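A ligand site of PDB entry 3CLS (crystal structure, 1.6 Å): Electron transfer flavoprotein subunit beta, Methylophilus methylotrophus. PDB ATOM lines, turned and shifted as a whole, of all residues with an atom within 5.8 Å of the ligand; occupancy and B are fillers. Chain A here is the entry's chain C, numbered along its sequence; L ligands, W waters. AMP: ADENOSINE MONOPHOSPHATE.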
ATOM      1  N   ALA A   6      -3.400  -2.919 -18.301  1.00  0.00           N
ATOM      2  CA  ALA A   6      -4.480  -2.318 -19.097  1.00  0.00           C
ATOM      3  C   ALA A   6      -5.180  -1.270 -18.223  1.00  0.00           C
ATOM      4  O   ALA A   6      -5.535  -1.577 -17.107  1.00  0.00           O
ATOM      5  CB  ALA A   6      -5.518  -3.382 -19.539  1.00  0.00           C
ATOM      6  N   VAL A   7      -5.307  -0.031 -18.714  1.00  0.00           N
ATOM      7  CA  VAL A   7      -5.911   1.020 -17.917  1.00  0.00           C
ATOM      8  C   VAL A   7      -7.019   1.707 -18.699  1.00  0.00           C
ATOM      9  O   VAL A   7      -6.942   1.809 -19.948  1.00  0.00           O
ATOM     10  CB  VAL A   7      -4.876   2.046 -17.373  1.00  0.00           C
ATOM     11  CG1 VAL A   7      -3.771   1.398 -16.615  1.00  0.00           C
ATOM     12  CG2 VAL A   7      -4.302   2.900 -18.494  1.00  0.00           C
ATOM     13  N   LYS A   8      -8.008   2.200 -17.964  1.00  0.00           N
ATOM     14  CA  LYS A   8      -9.154   2.904 -18.550  1.00  0.00           C
ATOM     15  C   LYS A   8      -9.265   4.309 -17.932  1.00  0.00           C
ATOM     16  O   LYS A   8      -9.166   4.473 -16.723  1.00  0.00           O
ATOM     17  CB  LYS A   8     -10.435   2.151 -18.272  1.00  0.00           C
ATOM     18  CG  LYS A   8     -11.616   2.831 -18.984  1.00  0.00           C
ATOM     19  CD  LYS A   8     -12.928   2.160 -18.657  1.00  0.00           C
ATOM     20  CE  LYS A   8     -14.113   2.764 -19.363  1.00  0.00           C
ATOM     21  NZ  LYS A   8     -15.476   2.173 -19.022  1.00  0.00           N
ATOM     22  N   ASN A  36      -9.250   5.348 -13.980  1.00  0.00           N
ATOM     23  CA  ASN A  36     -10.067   4.431 -13.172  1.00  0.00           C
ATOM     24  C   ASN A  36      -9.374   4.158 -11.854  1.00  0.00           C
ATOM     25  O   ASN A  36      -8.171   3.842 -11.838  1.00  0.00           O
ATOM     26  CB  ASN A  36     -10.289   3.146 -13.936  1.00  0.00           C
ATOM     27  CG  ASN A  36     -11.248   2.197 -13.228  1.00  0.00           C
ATOM     28  OD1 ASN A  36     -12.230   2.626 -12.566  1.00  0.00           O
ATOM     29  ND2 ASN A  36     -10.979   0.927 -13.406  1.00  0.00           N
ATOM     30  N   TRP A  38      -9.367   1.649  -9.868  1.00  0.00           N
ATOM     31  CA  TRP A  38      -8.763   0.287  -9.731  1.00  0.00           C
ATOM     32  C   TRP A  38      -7.409   0.305 -10.421  1.00  0.00           C
ATOM     33  O   TRP A  38      -6.448  -0.416 -10.023  1.00  0.00           O
ATOM     34  CB  TRP A  38      -9.671  -0.744 -10.385  1.00  0.00           C
ATOM     35  CG  TRP A  38     -10.745  -1.226  -9.421  1.00  0.00           C
ATOM     36  CD1 TRP A  38     -10.670  -2.274  -8.593  1.00  0.00           C
ATOM     37  CD2 TRP A  38     -11.981  -0.566  -9.133  1.00  0.00           C
ATOM     38  NE1 TRP A  38     -11.793  -2.374  -7.812  1.00  0.00           N
ATOM     39  CE2 TRP A  38     -12.636  -1.350  -8.126  1.00  0.00           C
ATOM     40  CE3 TRP A  38     -12.634   0.549  -9.641  1.00  0.00           C
ATOM     41  CZ2 TRP A  38     -13.829  -0.961  -7.586  1.00  0.00           C
ATOM     42  CZ3 TRP A  38     -13.827   0.914  -9.120  1.00  0.00           C
ATOM     43  CH2 TRP A  38     -14.427   0.149  -8.128  1.00  0.00           C
ATOM     44  N   ASP A  39      -7.269   1.148 -11.447  1.00  0.00           N
ATOM     45  CA  ASP A  39      -5.982   1.181 -12.168  1.00  0.00           C
ATOM     46  C   ASP A  39      -4.818   1.814 -11.389  1.00  0.00           C
ATOM     47  O   ASP A  39      -3.614   1.489 -11.621  1.00  0.00           O
ATOM     48  CB  ASP A  39      -6.145   1.833 -13.526  1.00  0.00           C
ATOM     49  CG  ASP A  39      -7.059   1.030 -14.448  1.00  0.00           C
ATOM     50  OD1 ASP A  39      -7.006  -0.233 -14.341  1.00  0.00           O
ATOM     51  OD2 ASP A  39      -7.763   1.724 -15.234  1.00  0.00           O
ATOM     52  N   VAL A  62      -1.427   0.306 -21.154  1.00  0.00           N
ATOM     53  CA  VAL A  62      -2.104   0.291 -22.448  1.00  0.00           C
ATOM     54  C   VAL A  62      -3.536   0.694 -22.228  1.00  0.00           C
ATOM     55  O   VAL A  62      -4.208   0.174 -21.400  1.00  0.00           O
ATOM     56  CB  VAL A  62      -2.067  -1.090 -23.119  1.00  0.00           C
ATOM     57  CG1 VAL A  62      -2.794  -1.102 -24.472  1.00  0.00           C
ATOM     58  CG2 VAL A  62      -0.616  -1.514 -23.266  1.00  0.00           C
ATOM     59  N   SER A  63      -4.046   1.574 -23.082  1.00  0.00           N
ATOM     60  CA  SER A  63      -5.477   2.007 -23.000  1.00  0.00           C
ATOM     61  C   SER A  63      -6.046   2.065 -24.389  1.00  0.00           C
ATOM     62  O   SER A  63      -5.393   2.511 -25.297  1.00  0.00           O
ATOM     63  CB  SER A  63      -5.677   3.372 -22.332  1.00  0.00           C
ATOM     64  OG  SER A  63      -7.035   3.622 -21.998  1.00  0.00           O
ATOM     65  N   VAL A  64      -7.295   1.622 -24.527  1.00  0.00           N
ATOM     66  CA  VAL A  64      -7.996   1.723 -25.782  1.00  0.00           C
ATOM     67  C   VAL A  64      -8.962   2.906 -25.601  1.00  0.00           C
ATOM     68  O   VAL A  64      -9.943   2.872 -24.800  1.00  0.00           O
ATOM     69  CB  VAL A  64      -8.804   0.487 -26.082  1.00  0.00           C
ATOM     70  CG1 VAL A  64      -9.597   0.668 -27.396  1.00  0.00           C
ATOM     71  CG2 VAL A  64      -7.945  -0.807 -26.128  1.00  0.00           C
ATOM     72  N   GLY A  65      -8.744   3.977 -26.324  1.00  0.00           N
ATOM     73  CA  GLY A  65      -9.596   5.119 -26.165  1.00  0.00           C
ATOM     74  C   GLY A  65      -9.139   6.304 -26.977  1.00  0.00           C
ATOM     75  O   GLY A  65      -8.054   6.314 -27.510  1.00  0.00           O
ATOM     76  N   ALA A  97     -17.029  -4.430 -23.342  1.00  0.00           N
ATOM     77  CA  ALA A  97     -15.907  -4.999 -22.584  1.00  0.00           C
ATOM     78  C   ALA A  97     -15.269  -6.079 -23.442  1.00  0.00           C
ATOM     79  O   ALA A  97     -14.091  -6.216 -23.421  1.00  0.00           O
ATOM     80  CB  ALA A  97     -16.347  -5.529 -21.301  1.00  0.00           C
ATOM     81  N   VAL A 100     -13.337  -4.574 -26.407  1.00  0.00           N
ATOM     82  CA  VAL A 100     -12.127  -4.009 -25.819  1.00  0.00           C
ATOM     83  C   VAL A 100     -11.129  -5.122 -25.466  1.00  0.00           C
ATOM     84  O   VAL A 100      -9.941  -4.978 -25.745  1.00  0.00           O
ATOM     85  CB  VAL A 100     -12.399  -2.983 -24.671  1.00  0.00           C
ATOM     86  CG1 VAL A 100     -11.118  -2.635 -23.871  1.00  0.00           C
ATOM     87  CG2 VAL A 100     -13.015  -1.760 -25.293  1.00  0.00           C
ATOM     88  N   LEU A 104      -7.308  -5.224 -26.841  1.00  0.00           N
ATOM     89  CA  LEU A 104      -6.181  -5.271 -25.906  1.00  0.00           C
ATOM     90  C   LEU A 104      -5.323  -6.490 -26.229  1.00  0.00           C
ATOM     91  O   LEU A 104      -4.082  -6.431 -26.244  1.00  0.00           O
ATOM     92  CB  LEU A 104      -6.711  -5.321 -24.482  1.00  0.00           C
ATOM     93  CG  LEU A 104      -7.224  -3.978 -23.941  1.00  0.00           C
ATOM     94  CD1 LEU A 104      -7.917  -4.240 -22.603  1.00  0.00           C
ATOM     95  CD2 LEU A 104      -6.034  -2.993 -23.680  1.00  0.00           C
ATOM     96  N   PHE A 117      -2.058  -7.196 -15.905  1.00  0.00           N
ATOM     97  CA  PHE A 117      -2.948  -6.753 -14.858  1.00  0.00           C
ATOM     98  C   PHE A 117      -4.087  -5.869 -15.410  1.00  0.00           C
ATOM     99  O   PHE A 117      -3.897  -4.990 -16.266  1.00  0.00           O
ATOM    100  CB  PHE A 117      -2.263  -5.899 -13.798  1.00  0.00           C
ATOM    101  CG  PHE A 117      -1.165  -6.604 -13.007  1.00  0.00           C
ATOM    102  CD1 PHE A 117      -1.017  -7.980 -12.973  1.00  0.00           C
ATOM    103  CD2 PHE A 117      -0.331  -5.804 -12.244  1.00  0.00           C
ATOM    104  CE1 PHE A 117       0.050  -8.548 -12.237  1.00  0.00           C
ATOM    105  CE2 PHE A 117       0.673  -6.340 -11.498  1.00  0.00           C
ATOM    106  CZ  PHE A 117       0.833  -7.717 -11.485  1.00  0.00           C
ATOM    107  N   ALA A 118      -5.273  -6.041 -14.858  1.00  0.00           N
ATOM    108  CA  ALA A 118      -6.422  -5.144 -15.176  1.00  0.00           C
ATOM    109  C   ALA A 118      -7.151  -4.886 -13.868  1.00  0.00           C
ATOM    110  O   ALA A 118      -6.960  -5.628 -12.914  1.00  0.00           O
ATOM    111  CB  ALA A 118      -7.372  -5.848 -16.157  1.00  0.00           C
ATOM    112  N   GLY A 119      -7.979  -3.827 -13.816  1.00  0.00           N
ATOM    113  CA  GLY A 119      -8.801  -3.527 -12.663  1.00  0.00           C
ATOM    114  C   GLY A 119      -9.925  -4.532 -12.551  1.00  0.00           C
ATOM    115  O   GLY A 119     -10.388  -5.057 -13.555  1.00  0.00           O
ATOM    116  N   VAL A 120     -10.365  -4.790 -11.312  1.00  0.00           N
ATOM    117  CA  VAL A 120     -11.604  -5.585 -11.129  1.00  0.00           C
ATOM    118  C   VAL A 120     -12.760  -5.028 -11.951  1.00  0.00           C
ATOM    119  O   VAL A 120     -13.501  -5.798 -12.559  1.00  0.00           O
ATOM    120  CB  VAL A 120     -12.027  -5.636  -9.645  1.00  0.00           C
ATOM    121  CG1 VAL A 120     -13.429  -6.149  -9.475  1.00  0.00           C
ATOM    122  CG2 VAL A 120     -11.113  -6.549  -8.934  1.00  0.00           C
ATOM    123  N   GLN A 121     -12.924  -3.704 -11.953  1.00  0.00           N
ATOM    124  CA  GLN A 121     -14.036  -3.116 -12.706  1.00  0.00           C
ATOM    125  C   GLN A 121     -13.751  -1.633 -12.951  1.00  0.00           C
ATOM    126  O   GLN A 121     -12.840  -1.062 -12.329  1.00  0.00           O
ATOM    127  CB  GLN A 121     -15.362  -3.255 -11.976  1.00  0.00           C
ATOM    128  CG  GLN A 121     -15.494  -2.468 -10.669  1.00  0.00           C
ATOM    129  CD  GLN A 121     -16.861  -2.631 -10.002  1.00  0.00           C
ATOM    130  OE1 GLN A 121     -17.439  -1.661  -9.509  1.00  0.00           O
ATOM    131  NE2 GLN A 121     -17.362  -3.837 -10.013  1.00  0.00           N
ATOM    132  N   SER A 122     -14.543  -1.043 -13.830  1.00  0.00           N
ATOM    133  CA  SER A 122     -14.467   0.421 -14.086  1.00  0.00           C
ATOM    134  C   SER A 122     -15.500   1.165 -13.231  1.00  0.00           C
ATOM    135  O   SER A 122     -16.614   0.706 -13.002  1.00  0.00           O
ATOM    136  CB  SER A 122     -14.756   0.747 -15.576  1.00  0.00           C
ATOM    137  OG  SER A 122     -15.932   0.089 -16.020  1.00  0.00           O
ATOM    138  N   GLN A 125     -18.855   2.222 -15.828  1.00  0.00           N
ATOM    139  CA  GLN A 125     -19.801   1.183 -16.291  1.00  0.00           C
ATOM    140  C   GLN A 125     -19.823  -0.034 -15.394  1.00  0.00           C
ATOM    141  O   GLN A 125     -20.770  -0.804 -15.411  1.00  0.00           O
ATOM    142  CB  GLN A 125     -19.438   0.749 -17.693  1.00  0.00           C
ATOM    143  CG  GLN A 125     -19.392   1.954 -18.709  1.00  0.00           C
ATOM    144  CD  GLN A 125     -20.302   3.313 -18.435  1.00  0.00           C
ATOM    145  OE1 GLN A 125     -21.281   3.345 -17.689  1.00  0.00           O
ATOM    146  NE2 GLN A 125     -19.919   4.409 -19.120  1.00  0.00           N
ATOM    147  N   ALA A 126     -18.728  -0.272 -14.700  1.00  0.00           N
ATOM    148  CA  ALA A 126     -18.666  -1.374 -13.718  1.00  0.00           C
ATOM    149  C   ALA A 126     -19.154  -2.666 -14.389  1.00  0.00           C
ATOM    150  O   ALA A 126     -20.040  -3.371 -13.849  1.00  0.00           O
ATOM    151  CB  ALA A 126     -19.501  -1.026 -12.534  1.00  0.00           C
ATOM    152  N   TYR A 127     -18.579  -2.972 -15.548  1.00  0.00           N
ATOM    153  CA  TYR A 127     -18.864  -4.262 -16.249  1.00  0.00           C
ATOM    154  C   TYR A 127     -18.261  -5.469 -15.486  1.00  0.00           C
ATOM    155  O   TYR A 127     -18.825  -6.575 -15.500  1.00  0.00           O
ATOM    156  CB  TYR A 127     -18.331  -4.229 -17.672  1.00  0.00           C
ATOM    157  CG  TYR A 127     -18.883  -3.216 -18.602  1.00  0.00           C
ATOM    158  CD1 TYR A 127     -18.034  -2.378 -19.296  1.00  0.00           C
ATOM    159  CD2 TYR A 127     -20.264  -3.039 -18.788  1.00  0.00           C
ATOM    160  CE1 TYR A 127     -18.479  -1.485 -20.192  1.00  0.00           C
ATOM    161  CE2 TYR A 127     -20.736  -2.110 -19.680  1.00  0.00           C
ATOM    162  CZ  TYR A 127     -19.825  -1.275 -20.323  1.00  0.00           C
ATOM    163  OH  TYR A 127     -20.206  -0.271 -21.212  1.00  0.00           O
ATOM    164  N   ALA A 128     -17.093  -5.244 -14.871  1.00  0.00           N
ATOM    165  CA  ALA A 128     -16.235  -6.310 -14.262  1.00  0.00           C
ATOM    166  C   ALA A 128     -16.087  -7.439 -15.278  1.00  0.00           C
ATOM    167  O   ALA A 128     -16.305  -8.632 -14.942  1.00  0.00           O
ATOM    168  CB  ALA A 128     -16.814  -6.824 -12.935  1.00  0.00           C
ATOM    169  N   SER A 129     -15.758  -7.066 -16.529  1.00  0.00           N
ATOM    170  CA  SER A 129     -15.640  -8.060 -17.628  1.00  0.00           C
ATOM    171  C   SER A 129     -14.372  -7.986 -18.460  1.00  0.00           C
ATOM    172  O   SER A 129     -13.986  -8.959 -19.092  1.00  0.00           O
ATOM    173  CB  SER A 129     -16.789  -7.807 -18.588  1.00  0.00           C
ATOM    174  OG  SER A 129     -18.018  -8.174 -17.964  1.00  0.00           O
ATOM    175  N   THR A 130     -13.801  -6.791 -18.574  1.00  0.00           N
ATOM    176  CA  THR A 130     -12.761  -6.550 -19.603  1.00  0.00           C
ATOM    177  C   THR A 130     -11.479  -7.418 -19.405  1.00  0.00           C
ATOM    178  O   THR A 130     -11.028  -8.089 -20.337  1.00  0.00           O
ATOM    179  CB  THR A 130     -12.432  -5.071 -19.712  1.00  0.00           C
ATOM    180  OG1 THR A 130     -13.647  -4.325 -19.948  1.00  0.00           O
ATOM    181  CG2 THR A 130     -11.442  -4.824 -20.771  1.00  0.00           C
ATOM    182  N   GLY A 131     -10.948  -7.439 -18.189  1.00  0.00           N
ATOM    183  CA  GLY A 131      -9.702  -8.147 -17.977  1.00  0.00           C
ATOM    184  C   GLY A 131      -9.843  -9.655 -18.223  1.00  0.00           C
ATOM    185  O   GLY A 131      -8.961 -10.307 -18.819  1.00  0.00           O
HETATM  186  P   AMP L   1     -14.543  -3.238 -16.663  1.00  0.00           P
HETATM  187  O1P AMP L   1     -14.273  -2.300 -17.785  1.00  0.00           O
HETATM  188  O2P AMP L   1     -14.747  -4.630 -17.140  1.00  0.00           O
HETATM  189  O3P AMP L   1     -15.531  -2.872 -15.704  1.00  0.00           O
HETATM  190  O5' AMP L   1     -13.103  -3.190 -15.905  1.00  0.00           O
HETATM  191  C5' AMP L   1     -12.247  -2.101 -15.896  1.00  0.00           C
HETATM  192  C4' AMP L   1     -10.821  -2.662 -16.160  1.00  0.00           C
HETATM  193  O4' AMP L   1     -10.673  -3.251 -17.455  1.00  0.00           O
HETATM  194  C3' AMP L   1      -9.884  -1.488 -16.078  1.00  0.00           C
HETATM  195  O3' AMP L   1      -9.319  -1.197 -14.781  1.00  0.00           O
HETATM  196  C2' AMP L   1      -8.858  -1.855 -17.113  1.00  0.00           C
HETATM  197  O2' AMP L   1      -7.871  -2.726 -16.525  1.00  0.00           O
HETATM  198  C1' AMP L   1      -9.666  -2.615 -18.142  1.00  0.00           C
HETATM  199  N9  AMP L   1     -10.271  -1.749 -19.168  1.00  0.00           N
HETATM  200  C8  AMP L   1     -11.581  -1.475 -19.381  1.00  0.00           C
HETATM  201  N7  AMP L   1     -11.700  -0.715 -20.463  1.00  0.00           N
HETATM  202  C5  AMP L   1     -10.488  -0.478 -20.927  1.00  0.00           C
HETATM  203  C6  AMP L   1      -9.936   0.335 -22.010  1.00  0.00           C
HETATM  204  N6  AMP L   1     -10.848   0.988 -22.813  1.00  0.00           N
HETATM  205  N1  AMP L   1      -8.625   0.280 -22.241  1.00  0.00           N
HETATM  206  C2  AMP L   1      -7.766  -0.408 -21.409  1.00  0.00           C
HETATM  207  N3  AMP L   1      -8.195  -1.133 -20.365  1.00  0.00           N
HETATM  208  C4  AMP L   1      -9.524  -1.178 -20.098  1.00  0.00           C
HETATM  209  O   HOH W   1     -15.274  -0.534 -19.386  1.00  0.00           O
HETATM  210  O   HOH W   2     -12.718   2.357 -25.404  1.00  0.00           O
HETATM  211  O   HOH W   3     -14.020  -2.003 -21.622  1.00  0.00           O
HETATM  212  O   HOH W   4      -5.211  -2.140 -14.503  1.00  0.00           O
HETATM  213  O   HOH W   5     -13.704   1.494 -23.001  1.00  0.00           O
HETATM  214  O   HOH W   6     -12.022  -6.097 -15.732  1.00  0.00           O
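OD1 of Asp 39 is in hydrogen-bond range of O3' of the ligand (2.5 Å). The backbone carbonyl oxygen (O) of Ala 6 lies within hydrogen-bond range of an oxygen (O2') of the ligand, 2.7 Å away. An oxygen (O2P) of the ligand lies within hydrogen-bond range of the backbone NH (N) of Ser 129. The backbone NH (N) of Thr 130 lies within hydrogen-bond range of an oxygen (O2P) of the ligand (2.8 Å). The side-chain hydroxyl (OG1) of Thr 130 lies within hydrogen-bond range of an oxygen (O1P) of the ligand (3.0 Å). An oxygen (O3P) of the ligand sits at hydrogen-bond distance from the backbone NH (N) of Ser 122. OG of Ser 122 is in hydrogen-bond range of O3P of the ligand. The backbone NH (N) of Val 64 lies within hydrogen-bond range of a nitrogen (N1) of the ligand, at 3.0 Å. O of Val 64 sits at hydrogen-bond distance from N6 of the ligand (2.9 Å). O2' of the ligand sits at hydrogen-bond distance from N of Gly 119. The backbone NH of Ala 128 lies within hydrogen-bond range of an oxygen (O3P) of the ligand (3.0 Å). The side-chain amide nitrogen (ND2) of Asn 36 is in hydrogen-bond range of an oxygen (O3') of the ligand (3.0 Å). An oxygen (O3P) of the ligand sits at hydrogen-bond distance from the backbone NH (N) of Tyr 127.
The side-chain carboxylate of Asp 39 is in hydrogen-bond range of the backbone NH of Lys 8 (2.8 Å). The backbone NH (N) of Ala 6 lies within hydrogen-bond range of the backbone carbonyl oxygen (O) of Phe 117 (2.9 Å). The backbone carbonyl oxygen of Tyr 127 lies within hydrogen-bond range of the side-chain hydroxyl of Ser 129. The backbone NH (N) of Val 7 is in hydrogen-bond range of the backbone carbonyl oxygen (O) of Val 62 (2.9 Å). The side-chain hydroxyl of Ser 63 sits at hydrogen-bond distance from the backbone carbonyl oxygen of Val 7. The side-chain hydroxyl of Ser 122 lies within hydrogen-bond range of the backbone NH of Ala 126, 3.1 Å away. O of Gln 121 is in hydrogen-bond range of ND2 of Asn 36, 2.9 Å away. The backbone carbonyl oxygen of Lys 8 lies within hydrogen-bond range of the backbone NH of Asn 36, 2.9 Å away.
The backbone carbonyl oxygen (O) of Val 7 lies close to a nitrogen (N3) of the ligand. Residues that only touch the ligand: Ala 118, Gln 121, Val 62, Lys 8, Ser 63, Val 100, Leu 104 and Ala 126. Of the 26 residues printed, 19 come within 4 Å of the ligand.
Water W1 lies within hydrogen-bond range of O1P of the ligand (2.6 Å), NZ of Lys 8 (2.7 Å) and OG of Ser 122 (3.5 Å). Water W3 bridges OG1 of Thr 130 and N7 of the ligand. Water W6 lies within hydrogen-bond range of the backbone carbonyl oxygen of Gly 119, the backbone NH of Gly 131, an oxygen (O5') of the ligand and the backbone NH of Thr 130. Water W4 lies within hydrogen-bond range of OD1 of Asp 39 (2.6 Å), O of Ala 6 (2.7 Å), N of Gly 119 (3.3 Å) and O2' of the ligand (3.4 Å). Water W2 bridges the backbone carbonyl oxygen (O) of Val 64 (2.9 Å) and a nitrogen (N6) of the ligand (3.5 Å).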
